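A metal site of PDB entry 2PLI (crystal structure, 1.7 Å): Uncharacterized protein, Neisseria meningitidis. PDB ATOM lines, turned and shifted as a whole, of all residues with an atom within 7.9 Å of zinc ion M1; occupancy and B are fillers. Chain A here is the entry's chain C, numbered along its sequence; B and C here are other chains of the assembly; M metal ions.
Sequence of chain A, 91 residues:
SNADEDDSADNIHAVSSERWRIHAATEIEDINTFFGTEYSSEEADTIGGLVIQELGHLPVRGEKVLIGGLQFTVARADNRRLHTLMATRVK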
ATOM      1  N   ASP A  10      22.511  19.788 -31.608  1.00  0.00           N
ATOM      2  CA  ASP A  10      22.268  18.428 -32.155  1.00  0.00           C
ATOM      3  C   ASP A  10      21.704  18.440 -33.600  1.00  0.00           C
ATOM      4  O   ASP A  10      20.591  18.939 -33.886  1.00  0.00           O
ATOM      5  CB  ASP A  10      21.338  17.662 -31.210  1.00  0.00           C
ATOM      6  CG  ASP A  10      20.117  18.443 -30.862  1.00  0.00           C
ATOM      7  OD1 ASP A  10      20.178  19.692 -30.836  1.00  0.00           O
ATOM      8  OD2 ASP A  10      19.119  17.825 -30.630  1.00  0.00           O
ATOM      9  N   ASN A  11      22.503  17.894 -34.517  1.00  0.00           N
ATOM     10  CA  ASN A  11      22.079  17.711 -35.893  1.00  0.00           C
ATOM     11  C   ASN A  11      21.033  16.622 -35.996  1.00  0.00           C
ATOM     12  O   ASN A  11      20.327  16.545 -37.007  1.00  0.00           O
ATOM     13  CB  ASN A  11      23.269  17.340 -36.764  1.00  0.00           C
ATOM     14  CG  ASN A  11      24.123  18.519 -37.108  1.00  0.00           C
ATOM     15  OD1 ASN A  11      23.641  19.648 -37.257  1.00  0.00           O
ATOM     16  ND2 ASN A  11      25.431  18.257 -37.282  1.00  0.00           N
ATOM     17  N   ILE A  12      20.956  15.759 -34.989  1.00  0.00           N
ATOM     18  CA  ILE A  12      19.972  14.692 -34.928  1.00  0.00           C
ATOM     19  C   ILE A  12      19.249  14.852 -33.572  1.00  0.00           C
ATOM     20  O   ILE A  12      19.828  14.638 -32.491  1.00  0.00           O
ATOM     21  CB  ILE A  12      20.594  13.268 -35.017  1.00  0.00           C
ATOM     22  CG1 ILE A  12      21.450  13.129 -36.285  1.00  0.00           C
ATOM     23  CG2 ILE A  12      19.470  12.216 -34.993  1.00  0.00           C
ATOM     24  CD1 ILE A  12      22.254  11.834 -36.353  1.00  0.00           C
ATOM     25  N   HIS A  13      18.015  15.308 -33.676  1.00  0.00           N
ATOM     26  CA  HIS A  13      17.172  15.655 -32.524  1.00  0.00           C
ATOM     27  C   HIS A  13      16.003  14.703 -32.478  1.00  0.00           C
ATOM     28  O   HIS A  13      15.210  14.590 -33.470  1.00  0.00           O
ATOM     29  CB  HIS A  13      16.645  17.079 -32.738  1.00  0.00           C
ATOM     30  CG  HIS A  13      15.581  17.486 -31.779  1.00  0.00           C
ATOM     31  ND1 HIS A  13      15.844  18.178 -30.615  1.00  0.00           N
ATOM     32  CD2 HIS A  13      14.242  17.328 -31.841  1.00  0.00           C
ATOM     33  CE1 HIS A  13      14.696  18.405 -29.987  1.00  0.00           C
ATOM     34  NE2 HIS A  13      13.713  17.870 -30.693  1.00  0.00           N
ATOM     35  N   ALA A  14      15.811  14.021 -31.363  1.00  0.00           N
ATOM     36  CA  ALA A  14      14.603  13.158 -31.189  1.00  0.00           C
ATOM     37  C   ALA A  14      13.384  14.011 -30.881  1.00  0.00           C
ATOM     38  O   ALA A  14      13.319  14.670 -29.837  1.00  0.00           O
ATOM     39  CB  ALA A  14      14.773  12.127 -30.096  1.00  0.00           C
ATOM     40  N   VAL A  15      12.449  14.025 -31.824  1.00  0.00           N
ATOM     41  CA  VAL A  15      11.141  14.622 -31.622  1.00  0.00           C
ATOM     42  C   VAL A  15      10.317  13.761 -30.642  1.00  0.00           C
ATOM     43  O   VAL A  15       9.665  14.277 -29.716  1.00  0.00           O
ATOM     44  CB  VAL A  15      10.439  14.797 -32.996  1.00  0.00           C
ATOM     45  CG1 VAL A  15       8.999  15.122 -32.837  1.00  0.00           C
ATOM     46  CG2 VAL A  15      11.142  15.938 -33.810  1.00  0.00           C
ATOM     47  N   ARG A  21      14.409  14.477 -36.039  1.00  0.00           N
ATOM     48  CA  ARG A  21      14.538  15.629 -36.913  1.00  0.00           C
ATOM     49  C   ARG A  21      16.023  15.780 -37.210  1.00  0.00           C
ATOM     50  O   ARG A  21      16.838  15.905 -36.274  1.00  0.00           O
ATOM     51  CB  ARG A  21      14.016  16.897 -36.260  1.00  0.00           C
ATOM     52  CG  ARG A  21      14.376  18.182 -36.999  1.00  0.00           C
ATOM     53  CD  ARG A  21      13.657  19.358 -36.359  1.00  0.00           C
ATOM     54  NE  ARG A  21      14.252  19.783 -35.109  1.00  0.00           N
ATOM     55  CZ  ARG A  21      13.592  20.009 -33.977  1.00  0.00           C
ATOM     56  NH1 ARG A  21      12.296  19.812 -33.855  1.00  0.00           N
ATOM     57  NH2 ARG A  21      14.256  20.470 -32.924  1.00  0.00           N
ATOM     58  N   ASN B  11      11.760  24.763 -22.215  1.00  0.00           N
ATOM     59  CA  ASN B  11      12.531  25.763 -22.932  1.00  0.00           C
ATOM     60  C   ASN B  11      11.758  27.013 -23.295  1.00  0.00           C
ATOM     61  O   ASN B  11      12.329  28.081 -23.455  1.00  0.00           O
ATOM     62  CB  ASN B  11      13.095  25.162 -24.221  1.00  0.00           C
ATOM     63  CG  ASN B  11      14.267  24.253 -23.986  1.00  0.00           C
ATOM     64  OD1 ASN B  11      14.392  23.226 -24.662  1.00  0.00           O
ATOM     65  ND2 ASN B  11      15.149  24.612 -23.058  1.00  0.00           N
ATOM     66  N   ALA B  25      18.857  28.822 -26.207  1.00  0.00           N
ATOM     67  CA  ALA B  25      19.300  27.567 -26.875  1.00  0.00           C
ATOM     68  C   ALA B  25      18.205  26.763 -27.575  1.00  0.00           C
ATOM     69  O   ALA B  25      18.497  25.774 -28.226  1.00  0.00           O
ATOM     70  CB  ALA B  25      20.032  26.623 -25.884  1.00  0.00           C
ATOM     71  N   THR B  26      16.966  27.208 -27.432  1.00  0.00           N
ATOM     72  CA  THR B  26      15.813  26.503 -27.982  1.00  0.00           C
ATOM     73  C   THR B  26      16.011  26.399 -29.501  1.00  0.00           C
ATOM     74  O   THR B  26      16.328  27.417 -30.162  1.00  0.00           O
ATOM     75  CB  THR B  26      14.496  27.243 -27.693  1.00  0.00           C
ATOM     76  OG1 THR B  26      14.348  27.398 -26.270  1.00  0.00           O
ATOM     77  CG2 THR B  26      13.299  26.451 -28.238  1.00  0.00           C
ATOM     78  N   GLU B  27      15.834  25.201 -30.059  1.00  0.00           N
ATOM     79  CA  GLU B  27      16.028  25.011 -31.509  1.00  0.00           C
ATOM     80  C   GLU B  27      14.939  25.690 -32.314  1.00  0.00           C
ATOM     81  O   GLU B  27      13.783  25.708 -31.930  1.00  0.00           O
ATOM     82  CB  GLU B  27      16.196  23.505 -31.890  1.00  0.00           C
ATOM     83  CG  GLU B  27      17.425  22.878 -31.195  1.00  0.00           C
ATOM     84  CD  GLU B  27      17.370  21.346 -31.092  1.00  0.00           C
ATOM     85  OE1 GLU B  27      17.087  20.791 -32.176  1.00  0.00           O
ATOM     86  OE2 GLU B  27      17.667  20.675 -30.025  1.00  0.00           O
ATOM     87  N   GLU B  29      13.410  24.976 -35.007  1.00  0.00           N
ATOM     88  CA  GLU B  29      12.281  24.178 -35.417  1.00  0.00           C
ATOM     89  C   GLU B  29      11.265  24.052 -34.291  1.00  0.00           C
ATOM     90  O   GLU B  29      10.066  23.934 -34.561  1.00  0.00           O
ATOM     91  CB  GLU B  29      12.696  22.816 -35.910  1.00  0.00           C
ATOM     92  CG  GLU B  29      13.777  22.904 -37.008  1.00  0.00           C
ATOM     93  CD  GLU B  29      15.211  22.794 -36.526  1.00  0.00           C
ATOM     94  OE1 GLU B  29      15.562  23.267 -35.442  1.00  0.00           O
ATOM     95  OE2 GLU B  29      16.076  22.170 -37.266  1.00  0.00           O
ATOM     96  N   ASP B  30      11.738  24.023 -33.052  1.00  0.00           N
ATOM     97  CA  ASP B  30      10.819  23.938 -31.910  1.00  0.00           C
ATOM     98  C   ASP B  30      10.036  25.248 -31.678  1.00  0.00           C
ATOM     99  O   ASP B  30       8.872  25.217 -31.260  1.00  0.00           O
ATOM    100  CB  ASP B  30      11.552  23.425 -30.677  1.00  0.00           C
ATOM    101  CG  ASP B  30      11.978  21.969 -30.875  1.00  0.00           C
ATOM    102  OD1 ASP B  30      11.183  21.152 -31.435  1.00  0.00           O
ATOM    103  OD2 ASP B  30      13.112  21.673 -30.536  1.00  0.00           O
ATOM    104  N   SER C   8      22.979  19.819 -25.042  1.00  0.00           N
ATOM    105  CA  SER C   8      21.897  20.398 -25.905  1.00  0.00           C
ATOM    106  C   SER C   8      20.806  20.953 -25.000  1.00  0.00           C
ATOM    107  O   SER C   8      20.904  20.847 -23.791  1.00  0.00           O
ATOM    108  CB  SER C   8      21.344  19.346 -26.883  1.00  0.00           C
ATOM    109  OG  SER C   8      20.192  18.681 -26.378  1.00  0.00           O
ATOM    110  N   ALA C   9      19.747  21.516 -25.587  1.00  0.00           N
ATOM    111  CA  ALA C   9      18.671  22.092 -24.774  1.00  0.00           C
ATOM    112  C   ALA C   9      17.504  21.100 -24.580  1.00  0.00           C
ATOM    113  O   ALA C   9      16.515  21.439 -23.953  1.00  0.00           O
ATOM    114  CB  ALA C   9      18.176  23.362 -25.372  1.00  0.00           C
ATOM    115  N   ASP C  10      17.648  19.887 -25.082  1.00  0.00           N
ATOM    116  CA  ASP C  10      16.610  18.872 -25.021  1.00  0.00           C
ATOM    117  C   ASP C  10      16.409  18.419 -23.570  1.00  0.00           C
ATOM    118  O   ASP C  10      17.380  17.949 -22.947  1.00  0.00           O
ATOM    119  CB  ASP C  10      17.052  17.598 -25.796  1.00  0.00           C
ATOM    120  CG  ASP C  10      17.370  17.818 -27.264  1.00  0.00           C
ATOM    121  OD1 ASP C  10      17.204  18.929 -27.783  1.00  0.00           O
ATOM    122  OD2 ASP C  10      17.838  16.852 -27.919  1.00  0.00           O
ATOM    123  N   ASN C  11      15.183  18.460 -23.031  1.00  0.00           N
ATOM    124  CA  ASN C  11      15.010  17.848 -21.709  1.00  0.00           C
ATOM    125  C   ASN C  11      15.100  16.320 -21.823  1.00  0.00           C
ATOM    126  O   ASN C  11      15.432  15.675 -20.868  1.00  0.00           O
ATOM    127  CB  ASN C  11      13.738  18.264 -20.980  1.00  0.00           C
ATOM    128  CG  ASN C  11      12.500  18.171 -21.795  1.00  0.00           C
ATOM    129  OD1 ASN C  11      12.412  17.442 -22.794  1.00  0.00           O
ATOM    130  ND2 ASN C  11      11.474  18.971 -21.366  1.00  0.00           N
ATOM    131  N   ILE C  12      14.761  15.790 -22.992  1.00  0.00           N
ATOM    132  CA  ILE C  12      14.901  14.366 -23.294  1.00  0.00           C
ATOM    133  C   ILE C  12      15.813  14.267 -24.497  1.00  0.00           C
ATOM    134  O   ILE C  12      15.364  14.533 -25.617  1.00  0.00           O
ATOM    135  CB  ILE C  12      13.545  13.680 -23.628  1.00  0.00           C
ATOM    136  CG1 ILE C  12      12.508  13.879 -22.517  1.00  0.00           C
ATOM    137  CG2 ILE C  12      13.743  12.181 -23.895  1.00  0.00           C
ATOM    138  CD1 ILE C  12      11.124  13.340 -22.834  1.00  0.00           C
ATOM    139  N   HIS C  13      17.073  13.925 -24.270  1.00  0.00           N
ATOM    140  CA  HIS C  13      18.109  14.054 -25.289  1.00  0.00           C
ATOM    141  C   HIS C  13      18.555  12.707 -25.747  1.00  0.00           C
ATOM    142  O   HIS C  13      19.041  11.928 -24.948  1.00  0.00           O
ATOM    143  CB  HIS C  13      19.293  14.768 -24.710  1.00  0.00           C
ATOM    144  CG  HIS C  13      20.373  14.989 -25.699  1.00  0.00           C
ATOM    145  ND1 HIS C  13      20.160  15.663 -26.877  1.00  0.00           N
ATOM    146  CD2 HIS C  13      21.673  14.624 -25.677  1.00  0.00           C
ATOM    147  CE1 HIS C  13      21.293  15.669 -27.572  1.00  0.00           C
ATOM    148  NE2 HIS C  13      22.209  15.041 -26.862  1.00  0.00           N
ATOM    149  N   ALA C  14      18.405  12.401 -27.015  1.00  0.00           N
ATOM    150  CA  ALA C  14      18.860  11.111 -27.499  1.00  0.00           C
ATOM    151  C   ALA C  14      20.379  11.168 -27.656  1.00  0.00           C
ATOM    152  O   ALA C  14      20.864  11.872 -28.539  1.00  0.00           O
ATOM    153  CB  ALA C  14      18.209  10.769 -28.833  1.00  0.00           C
HETATM  154 ZN    ZN M   1      17.587  18.729 -29.803  1.00  0.00          ZN
HETATM  155 ZN    ZN M   2      17.611  22.199 -36.001  1.00  0.00          ZN
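Within 4 Å of zinc ion M1: Asp 10 of chain A, His 13 of chain A, Glu 27 of chain B and Asp 10 of chain C.
The nearest printed residue that does not touch zinc ion M1 is Ser 8 of chain C (4.3 Å).
OE1 of Glu 27 of chain B lies within salt-bridge range of NH2 of Arg 21 (2.9 Å).
N of Arg 21 lies within hydrogen-bond range of O of His 13 of chain A, 2.7 Å away.
N of Asp 10 of chain C lies close to OG of Ser 8 of chain C (3.1 Å).
OD2 of Asp 10 of chain C is in hydrogen-bond range of ND1 of His 13 of chain C (2.8 Å).
Zinc ion M1 is bound by the side-chain carboxylate (OE2) of Glu 27 of chain B (2.0 Å), the side-chain carboxylate (OD2) of Asp 10 of chain A (2.0 Å), a ring nitrogen (ND1) of His 13 of chain A (2.0 Å) and the side-chain carboxylate (OD1) of Asp 10 of chain C (2.1 Å).
Slightly farther from zinc ion M1 lies the side-chain carboxylate (OD2) of Asp 10 of chain C (2.7 Å).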
